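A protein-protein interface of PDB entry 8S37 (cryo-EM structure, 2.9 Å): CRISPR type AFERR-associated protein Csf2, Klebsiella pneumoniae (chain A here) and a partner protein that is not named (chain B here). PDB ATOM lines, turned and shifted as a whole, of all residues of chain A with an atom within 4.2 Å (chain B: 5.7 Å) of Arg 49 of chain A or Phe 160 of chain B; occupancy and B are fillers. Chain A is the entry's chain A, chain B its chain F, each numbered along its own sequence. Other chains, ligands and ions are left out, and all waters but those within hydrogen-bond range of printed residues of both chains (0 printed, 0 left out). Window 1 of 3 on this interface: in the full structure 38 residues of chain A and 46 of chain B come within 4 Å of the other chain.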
ATOM      1  N   GLY A  45       8.823  19.546  15.975  1.00  0.00           N
ATOM      2  CA  GLY A  45       7.593  19.157  15.317  1.00  0.00           C
ATOM      3  C   GLY A  45       7.031  17.863  15.854  1.00  0.00           C
ATOM      4  O   GLY A  45       5.848  17.580  15.652  1.00  0.00           O
ATOM      5  N   THR A  46       7.849  17.088  16.568  1.00  0.00           N
ATOM      6  CA  THR A  46       7.364  15.858  17.177  1.00  0.00           C
ATOM      7  C   THR A  46       6.423  16.165  18.331  1.00  0.00           C
ATOM      8  O   THR A  46       5.380  15.520  18.476  1.00  0.00           O
ATOM      9  CB  THR A  46       8.539  15.013  17.664  1.00  0.00           C
ATOM     10  OG1 THR A  46       9.334  15.776  18.579  1.00  0.00           O
ATOM     11  CG2 THR A  46       9.399  14.578  16.497  1.00  0.00           C
ATOM     12  N   SER A  47       6.772  17.148  19.160  1.00  0.00           N
ATOM     13  CA  SER A  47       5.898  17.511  20.268  1.00  0.00           C
ATOM     14  C   SER A  47       4.574  18.063  19.760  1.00  0.00           C
ATOM     15  O   SER A  47       3.508  17.697  20.268  1.00  0.00           O
ATOM     16  CB  SER A  47       6.587  18.532  21.169  1.00  0.00           C
ATOM     17  OG  SER A  47       5.723  18.949  22.211  1.00  0.00           O
ATOM     18  N   ILE A  48       4.616  18.947  18.765  1.00  0.00           N
ATOM     19  CA  ILE A  48       3.372  19.488  18.230  1.00  0.00           C
ATOM     20  C   ILE A  48       2.562  18.380  17.571  1.00  0.00           C
ATOM     21  O   ILE A  48       1.334  18.330  17.704  1.00  0.00           O
ATOM     22  CB  ILE A  48       3.652  20.637  17.241  1.00  0.00           C
ATOM     23  CG1 ILE A  48       4.527  21.725  17.877  1.00  0.00           C
ATOM     24  CG2 ILE A  48       2.335  21.250  16.750  1.00  0.00           C
ATOM     25  CD1 ILE A  48       4.989  22.792  16.896  1.00  0.00           C
ATOM     26  N   ARG A  49       3.232  17.468  16.862  1.00  0.00           N
ATOM     27  CA  ARG A  49       2.516  16.378  16.214  1.00  0.00           C
ATOM     28  C   ARG A  49       1.834  15.489  17.239  1.00  0.00           C
ATOM     29  O   ARG A  49       0.678  15.100  17.061  1.00  0.00           O
ATOM     30  CB  ARG A  49       3.469  15.559  15.347  1.00  0.00           C
ATOM     31  CG  ARG A  49       2.759  14.593  14.414  1.00  0.00           C
ATOM     32  CD  ARG A  49       3.715  13.950  13.427  1.00  0.00           C
ATOM     33  NE  ARG A  49       3.022  13.463  12.241  1.00  0.00           N
ATOM     34  CZ  ARG A  49       2.242  12.391  12.207  1.00  0.00           C
ATOM     35  NH1 ARG A  49       2.001  11.672  13.291  1.00  0.00           N
ATOM     36  NH2 ARG A  49       1.685  12.032  11.054  1.00  0.00           N
ATOM     37  N   GLY A  50       2.529  15.167  18.328  1.00  0.00           N
ATOM     38  CA  GLY A  50       1.920  14.343  19.355  1.00  0.00           C
ATOM     39  C   GLY A  50       0.783  15.047  20.068  1.00  0.00           C
ATOM     40  O   GLY A  50      -0.247  14.437  20.359  1.00  0.00           O
ATOM     41  N   THR A  51       0.954  16.336  20.368  1.00  0.00           N
ATOM     42  CA  THR A  51      -0.121  17.087  21.007  1.00  0.00           C
ATOM     43  C   THR A  51      -1.357  17.130  20.122  1.00  0.00           C
ATOM     44  O   THR A  51      -2.481  16.934  20.599  1.00  0.00           O
ATOM     45  CB  THR A  51       0.348  18.502  21.333  1.00  0.00           C
ATOM     46  OG1 THR A  51       1.523  18.443  22.149  1.00  0.00           O
ATOM     47  CG2 THR A  51      -0.737  19.266  22.072  1.00  0.00           C
ATOM     48  N   LEU A  52      -1.170  17.361  18.823  1.00  0.00           N
ATOM     49  CA  LEU A  52      -2.321  17.429  17.934  1.00  0.00           C
ATOM     50  C   LEU A  52      -2.920  16.053  17.690  1.00  0.00           C
ATOM     51  O   LEU A  52      -4.134  15.936  17.504  1.00  0.00           O
ATOM     52  CB  LEU A  52      -1.924  18.092  16.617  1.00  0.00           C
ATOM     53  CG  LEU A  52      -1.660  19.596  16.729  1.00  0.00           C
ATOM     54  CD1 LEU A  52      -0.884  20.100  15.527  1.00  0.00           C
ATOM     55  CD2 LEU A  52      -2.964  20.362  16.877  1.00  0.00           C
ATOM     56  N   ARG A  53      -2.102  15.000  17.704  1.00  0.00           N
ATOM     57  CA  ARG A  53      -2.656  13.654  17.632  1.00  0.00           C
ATOM     58  C   ARG A  53      -3.485  13.341  18.867  1.00  0.00           C
ATOM     59  O   ARG A  53      -4.539  12.709  18.769  1.00  0.00           O
ATOM     60  CB  ARG A  53      -1.535  12.631  17.469  1.00  0.00           C
ATOM     61  CG  ARG A  53      -2.015  11.197  17.565  1.00  0.00           C
ATOM     62  CD  ARG A  53      -1.050  10.238  16.906  1.00  0.00           C
ATOM     63  NE  ARG A  53      -1.615   8.899  16.807  1.00  0.00           N
ATOM     64  CZ  ARG A  53      -1.130   7.929  16.045  1.00  0.00           C
ATOM     65  NH1 ARG A  53      -0.057   8.109  15.289  1.00  0.00           N
ATOM     66  NH2 ARG A  53      -1.740   6.748  16.035  1.00  0.00           N
ATOM     67  N   LEU A 115      -4.986  10.489   9.142  1.00  0.00           N
ATOM     68  CA  LEU A 115      -4.197  11.699   9.353  1.00  0.00           C
ATOM     69  C   LEU A 115      -2.853  11.364   9.981  1.00  0.00           C
ATOM     70  O   LEU A 115      -1.795  11.621   9.397  1.00  0.00           O
ATOM     71  CB  LEU A 115      -4.966  12.668  10.249  1.00  0.00           C
ATOM     72  CG  LEU A 115      -6.242  13.285   9.687  1.00  0.00           C
ATOM     73  CD1 LEU A 115      -7.018  13.971  10.799  1.00  0.00           C
ATOM     74  CD2 LEU A 115      -5.907  14.268   8.581  1.00  0.00           C
ATOM     75  N   PHE A 116      -2.881  10.778  11.172  1.00  0.00           N
ATOM     76  CA  PHE A 116      -1.685  10.300  11.849  1.00  0.00           C
ATOM     77  C   PHE A 116      -1.645   8.789  11.683  1.00  0.00           C
ATOM     78  O   PHE A 116      -2.573   8.092  12.103  1.00  0.00           O
ATOM     79  CB  PHE A 116      -1.700  10.677  13.329  1.00  0.00           C
ATOM     80  CG  PHE A 116      -2.060  12.112  13.587  1.00  0.00           C
ATOM     81  CD1 PHE A 116      -3.381  12.494  13.730  1.00  0.00           C
ATOM     82  CD2 PHE A 116      -1.077  13.076  13.698  1.00  0.00           C
ATOM     83  CE1 PHE A 116      -3.713  13.808  13.971  1.00  0.00           C
ATOM     84  CE2 PHE A 116      -1.405  14.392  13.941  1.00  0.00           C
ATOM     85  CZ  PHE A 116      -2.725  14.757  14.077  1.00  0.00           C
ATOM     86  N   VAL A 125      -0.591  13.525   7.926  1.00  0.00           N
ATOM     87  CA  VAL A 125      -0.286  14.811   8.536  1.00  0.00           C
ATOM     88  C   VAL A 125       1.213  14.871   8.794  1.00  0.00           C
ATOM     89  O   VAL A 125       1.746  14.108   9.607  1.00  0.00           O
ATOM     90  CB  VAL A 125      -1.078  15.015   9.832  1.00  0.00           C
ATOM     91  CG1 VAL A 125      -0.530  16.195  10.609  1.00  0.00           C
ATOM     92  CG2 VAL A 125      -2.542  15.222   9.518  1.00  0.00           C
ATOM     93  N   GLY A 126       1.887  15.782   8.101  1.00  0.00           N
ATOM     94  CA  GLY A 126       3.245  16.164   8.419  1.00  0.00           C
ATOM     95  C   GLY A 126       3.285  17.478   9.170  1.00  0.00           C
ATOM     96  O   GLY A 126       3.090  18.537   8.569  1.00  0.00           O
ATOM     97  N   ILE A 127       3.531  17.433  10.472  1.00  0.00           N
ATOM     98  CA  ILE A 127       3.517  18.617  11.321  1.00  0.00           C
ATOM     99  C   ILE A 127       4.957  19.071  11.520  1.00  0.00           C
ATOM    100  O   ILE A 127       5.728  18.435  12.245  1.00  0.00           O
ATOM    101  CB  ILE A 127       2.800  18.344  12.648  1.00  0.00           C
ATOM    102  CG1 ILE A 127       1.295  18.494  12.435  1.00  0.00           C
ATOM    103  CG2 ILE A 127       3.255  19.300  13.740  1.00  0.00           C
ATOM    104  CD1 ILE A 127       0.445  17.728  13.409  1.00  0.00           C
ATOM    105  N   GLU B  32       8.216  13.941  -3.444  1.00  0.00           N
ATOM    106  CA  GLU B  32       7.261  14.119  -2.355  1.00  0.00           C
ATOM    107  C   GLU B  32       6.509  15.435  -2.512  1.00  0.00           C
ATOM    108  O   GLU B  32       5.286  15.495  -2.320  1.00  0.00           O
ATOM    109  CB  GLU B  32       7.983  14.067  -1.010  1.00  0.00           C
ATOM    110  CG  GLU B  32       7.059  13.971   0.194  1.00  0.00           C
ATOM    111  CD  GLU B  32       6.289  12.667   0.240  1.00  0.00           C
ATOM    112  OE1 GLU B  32       6.737  11.688  -0.392  1.00  0.00           O
ATOM    113  OE2 GLU B  32       5.232  12.623   0.903  1.00  0.00           O
ATOM    114  N   GLN B  36       2.474  15.888  -3.119  1.00  0.00           N
ATOM    115  CA  GLN B  36       1.606  16.809  -2.399  1.00  0.00           C
ATOM    116  C   GLN B  36       0.951  17.815  -3.340  1.00  0.00           C
ATOM    117  O   GLN B  36      -0.217  18.167  -3.156  1.00  0.00           O
ATOM    118  CB  GLN B  36       2.407  17.553  -1.334  1.00  0.00           C
ATOM    119  CG  GLN B  36       2.846  16.703  -0.171  1.00  0.00           C
ATOM    120  CD  GLN B  36       3.692  17.481   0.810  1.00  0.00           C
ATOM    121  OE1 GLN B  36       3.225  18.433   1.432  1.00  0.00           O
ATOM    122  NE2 GLN B  36       4.951  17.089   0.942  1.00  0.00           N
ATOM    123  N   ARG B  85      12.471  10.256  19.060  1.00  0.00           N
ATOM    124  CA  ARG B  85      11.021  10.138  19.089  1.00  0.00           C
ATOM    125  C   ARG B  85      10.650   9.252  20.268  1.00  0.00           C
ATOM    126  O   ARG B  85      11.042   8.081  20.318  1.00  0.00           O
ATOM    127  CB  ARG B  85      10.500   9.566  17.775  1.00  0.00           C
ATOM    128  CG  ARG B  85      10.753  10.486  16.592  1.00  0.00           C
ATOM    129  CD  ARG B  85       9.471  10.913  15.906  1.00  0.00           C
ATOM    130  NE  ARG B  85       8.500  11.476  16.835  1.00  0.00           N
ATOM    131  CZ  ARG B  85       7.285  11.884  16.497  1.00  0.00           C
ATOM    132  NH1 ARG B  85       6.860  11.835  15.244  1.00  0.00           N
ATOM    133  NH2 ARG B  85       6.474  12.356  17.439  1.00  0.00           N
ATOM    134  N   HIS B 152       5.348  20.711   1.794  1.00  0.00           N
ATOM    135  CA  HIS B 152       5.793  20.302   3.125  1.00  0.00           C
ATOM    136  C   HIS B 152       6.783  19.146   2.998  1.00  0.00           C
ATOM    137  O   HIS B 152       6.492  17.987   3.295  1.00  0.00           O
ATOM    138  CB  HIS B 152       4.600  19.932   3.989  1.00  0.00           C
ATOM    139  CG  HIS B 152       4.940  19.742   5.430  1.00  0.00           C
ATOM    140  ND1 HIS B 152       5.277  20.792   6.257  1.00  0.00           N
ATOM    141  CD2 HIS B 152       5.000  18.628   6.194  1.00  0.00           C
ATOM    142  CE1 HIS B 152       5.529  20.332   7.469  1.00  0.00           C
ATOM    143  NE2 HIS B 152       5.369  19.021   7.457  1.00  0.00           N
ATOM    144  N   VAL B 153       7.980  19.495   2.538  1.00  0.00           N
ATOM    145  CA  VAL B 153       9.054  18.538   2.308  1.00  0.00           C
ATOM    146  C   VAL B 153      10.299  19.014   3.037  1.00  0.00           C
ATOM    147  O   VAL B 153      10.645  20.199   2.986  1.00  0.00           O
ATOM    148  CB  VAL B 153       9.344  18.354   0.806  1.00  0.00           C
ATOM    149  CG1 VAL B 153       8.118  17.819   0.101  1.00  0.00           C
ATOM    150  CG2 VAL B 153       9.806  19.662   0.171  1.00  0.00           C
ATOM    151  N   TYR B 157      14.852  11.691   6.698  1.00  0.00           N
ATOM    152  CA  TYR B 157      13.885  10.649   6.998  1.00  0.00           C
ATOM    153  C   TYR B 157      12.599  11.263   7.529  1.00  0.00           C
ATOM    154  O   TYR B 157      12.645  12.210   8.320  1.00  0.00           O
ATOM    155  CB  TYR B 157      14.471   9.675   8.017  1.00  0.00           C
ATOM    156  CG  TYR B 157      13.519   8.606   8.485  1.00  0.00           C
ATOM    157  CD1 TYR B 157      12.782   7.861   7.580  1.00  0.00           C
ATOM    158  CD2 TYR B 157      13.383   8.320   9.833  1.00  0.00           C
ATOM    159  CE1 TYR B 157      11.920   6.875   8.007  1.00  0.00           C
ATOM    160  CE2 TYR B 157      12.526   7.337  10.267  1.00  0.00           C
ATOM    161  CZ  TYR B 157      11.797   6.617   9.352  1.00  0.00           C
ATOM    162  OH  TYR B 157      10.944   5.633   9.789  1.00  0.00           O
ATOM    163  N   ASP B 158      11.471  10.772   7.018  1.00  0.00           N
ATOM    164  CA  ASP B 158      10.119  10.969   7.560  1.00  0.00           C
ATOM    165  C   ASP B 158       9.893  12.398   8.057  1.00  0.00           C
ATOM    166  O   ASP B 158       9.531  12.647   9.207  1.00  0.00           O
ATOM    167  CB  ASP B 158       9.784   9.918   8.634  1.00  0.00           C
ATOM    168  CG  ASP B 158      10.556  10.084   9.945  1.00  0.00           C
ATOM    169  OD1 ASP B 158      11.365  11.012  10.103  1.00  0.00           O
ATOM    170  OD2 ASP B 158      10.314   9.265  10.856  1.00  0.00           O
ATOM    171  N   TYR B 159      10.095  13.349   7.143  1.00  0.00           N
ATOM    172  CA  TYR B 159       9.900  14.747   7.500  1.00  0.00           C
ATOM    173  C   TYR B 159       8.469  15.017   7.935  1.00  0.00           C
ATOM    174  O   TYR B 159       8.227  15.919   8.742  1.00  0.00           O
ATOM    175  CB  TYR B 159      10.261  15.654   6.328  1.00  0.00           C
ATOM    176  CG  TYR B 159       9.810  17.079   6.536  1.00  0.00           C
ATOM    177  CD1 TYR B 159      10.433  17.893   7.467  1.00  0.00           C
ATOM    178  CD2 TYR B 159       8.750  17.604   5.816  1.00  0.00           C
ATOM    179  CE1 TYR B 159      10.024  19.192   7.666  1.00  0.00           C
ATOM    180  CE2 TYR B 159       8.335  18.905   6.005  1.00  0.00           C
ATOM    181  CZ  TYR B 159       8.974  19.694   6.935  1.00  0.00           C
ATOM    182  OH  TYR B 159       8.563  20.990   7.131  1.00  0.00           O
ATOM    183  N   PHE B 160       7.506  14.255   7.417  1.00  0.00           N
ATOM    184  CA  PHE B 160       6.138  14.399   7.895  1.00  0.00           C
ATOM    185  C   PHE B 160       6.050  14.082   9.382  1.00  0.00           C
ATOM    186  O   PHE B 160       5.611  14.910  10.186  1.00  0.00           O
ATOM    187  CB  PHE B 160       5.206  13.485   7.100  1.00  0.00           C
ATOM    188  CG  PHE B 160       4.901  13.981   5.721  1.00  0.00           C
ATOM    189  CD1 PHE B 160       5.850  13.903   4.720  1.00  0.00           C
ATOM    190  CD2 PHE B 160       3.661  14.515   5.422  1.00  0.00           C
ATOM    191  CE1 PHE B 160       5.571  14.357   3.449  1.00  0.00           C
ATOM    192  CE2 PHE B 160       3.377  14.971   4.155  1.00  0.00           C
ATOM    193  CZ  PHE B 160       4.333  14.890   3.167  1.00  0.00           C
ATOM    194  N   SER B 161       6.511  12.897   9.774  1.00  0.00           N
ATOM    195  CA  SER B 161       6.278  12.457  11.142  1.00  0.00           C
ATOM    196  C   SER B 161       7.251  13.106  12.121  1.00  0.00           C
ATOM    197  O   SER B 161       6.837  13.811  13.046  1.00  0.00           O
ATOM    198  CB  SER B 161       6.387  10.935  11.216  1.00  0.00           C
ATOM    199  OG  SER B 161       6.452  10.506  12.561  1.00  0.00           O
ATOM    200  N   ALA B 162       8.550  12.887  11.927  1.00  0.00           N
ATOM    201  CA  ALA B 162       9.526  13.386  12.885  1.00  0.00           C
ATOM    202  C   ALA B 162       9.879  14.852  12.689  1.00  0.00           C
ATOM    203  O   ALA B 162      10.530  15.432  13.564  1.00  0.00           O
ATOM    204  CB  ALA B 162      10.805  12.551  12.807  1.00  0.00           C
ATOM    205  N   ALA B 163       9.482  15.460  11.574  1.00  0.00           N
ATOM    206  CA  ALA B 163       9.831  16.846  11.275  1.00  0.00           C
ATOM    207  C   ALA B 163      11.342  17.010  11.154  1.00  0.00           C
ATOM    208  O   ALA B 163      11.895  18.047  11.525  1.00  0.00           O
ATOM    209  CB  ALA B 163       9.270  17.801  12.330  1.00  0.00           C
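Of the 12 printed residues of chain B, 6 touch a printed residue of chain A. Hydrophobic or aromatic side chains of chain B within 4 Å of the printed part of chain A: His 152, Phe 160 and Ala 163. Along chain A the printed residues that touch a printed residue of chain B span positions 45 to 127. Among the printed residues, 11 pairs touch across the chains.
The backbone NH (N) of Ile 127 of chain A is in hydrogen-bond range of the backbone carbonyl oxygen (O) of Phe 160 of chain B. The backbone carbonyl oxygen (O) of Gly 126 of chain A sits at hydrogen-bond distance from a ring nitrogen (NE2) of His 152 of chain B (2.6 Å).
ND1 of His 152 of chain B lies close to OH of Tyr 159 of chain B (3.4 Å). The backbone carbonyl oxygen (O) of Leu 115 of chain A sits at hydrogen-bond distance from the backbone NH (N) of Val 125 of chain A (2.7 Å). NH2 of Arg 49 of chain A is in hydrogen-bond range of O of Val 125 of chain A (2.5 Å). O of Ser 161 of chain B sits at hydrogen-bond distance from NH1 of Arg 85 of chain B. O of His 152 of chain B sits at hydrogen-bond distance from NE2 of Gln 36 of chain B.
Of chain B, only Phe 160 (3.6 Å) and Ser 161 (3.1 Å) come within 4 Å of Arg 49 of chain A. Of the printed residues of chain B, Ile 127 of chain A touches His 152, Phe 160 and Ala 163. Of the printed residues of chain A, His 152 of chain B touches Gly 126 (2.6 Å) and Ile 127 (3.9 Å). Tyr 157 of chain B touches none of the printed residues of chain A. Of the printed residues of chain A, Phe 160 of chain B touches Arg 49, Val 125, Gly 126 and Ile 127. The nearest printed residue of chain A that does not touch Arg 85 of chain B is Arg 49 of chain A (4.2 Å).
Gly 45 of chain A touches Ala 163 of chain B. CG2 of Thr 46 of chain A touches NE of Arg 85 of chain B, at 3.2 Å. CG2 of Thr 46 of chain A touches O of Ala 162 of chain B, 3.3 Å away. Phe 160 of chain B touches Arg 49 of chain A (O to NE, 3.6 Å). Arg 49 of chain A touches Ser 161 of chain B (CD to O, 3.1 Å). Val 125 of chain A touches Phe 160 of chain B (O to O, 3.99 Å). Phe 160 of chain B touches Gly 126 of chain A. NE2 of His 152 of chain B touches N of Ile 127 of chain A, 3.9 Å away. Ile 127 of chain A touches Ala 163 of chain B (O to CB, 3.6 Å).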
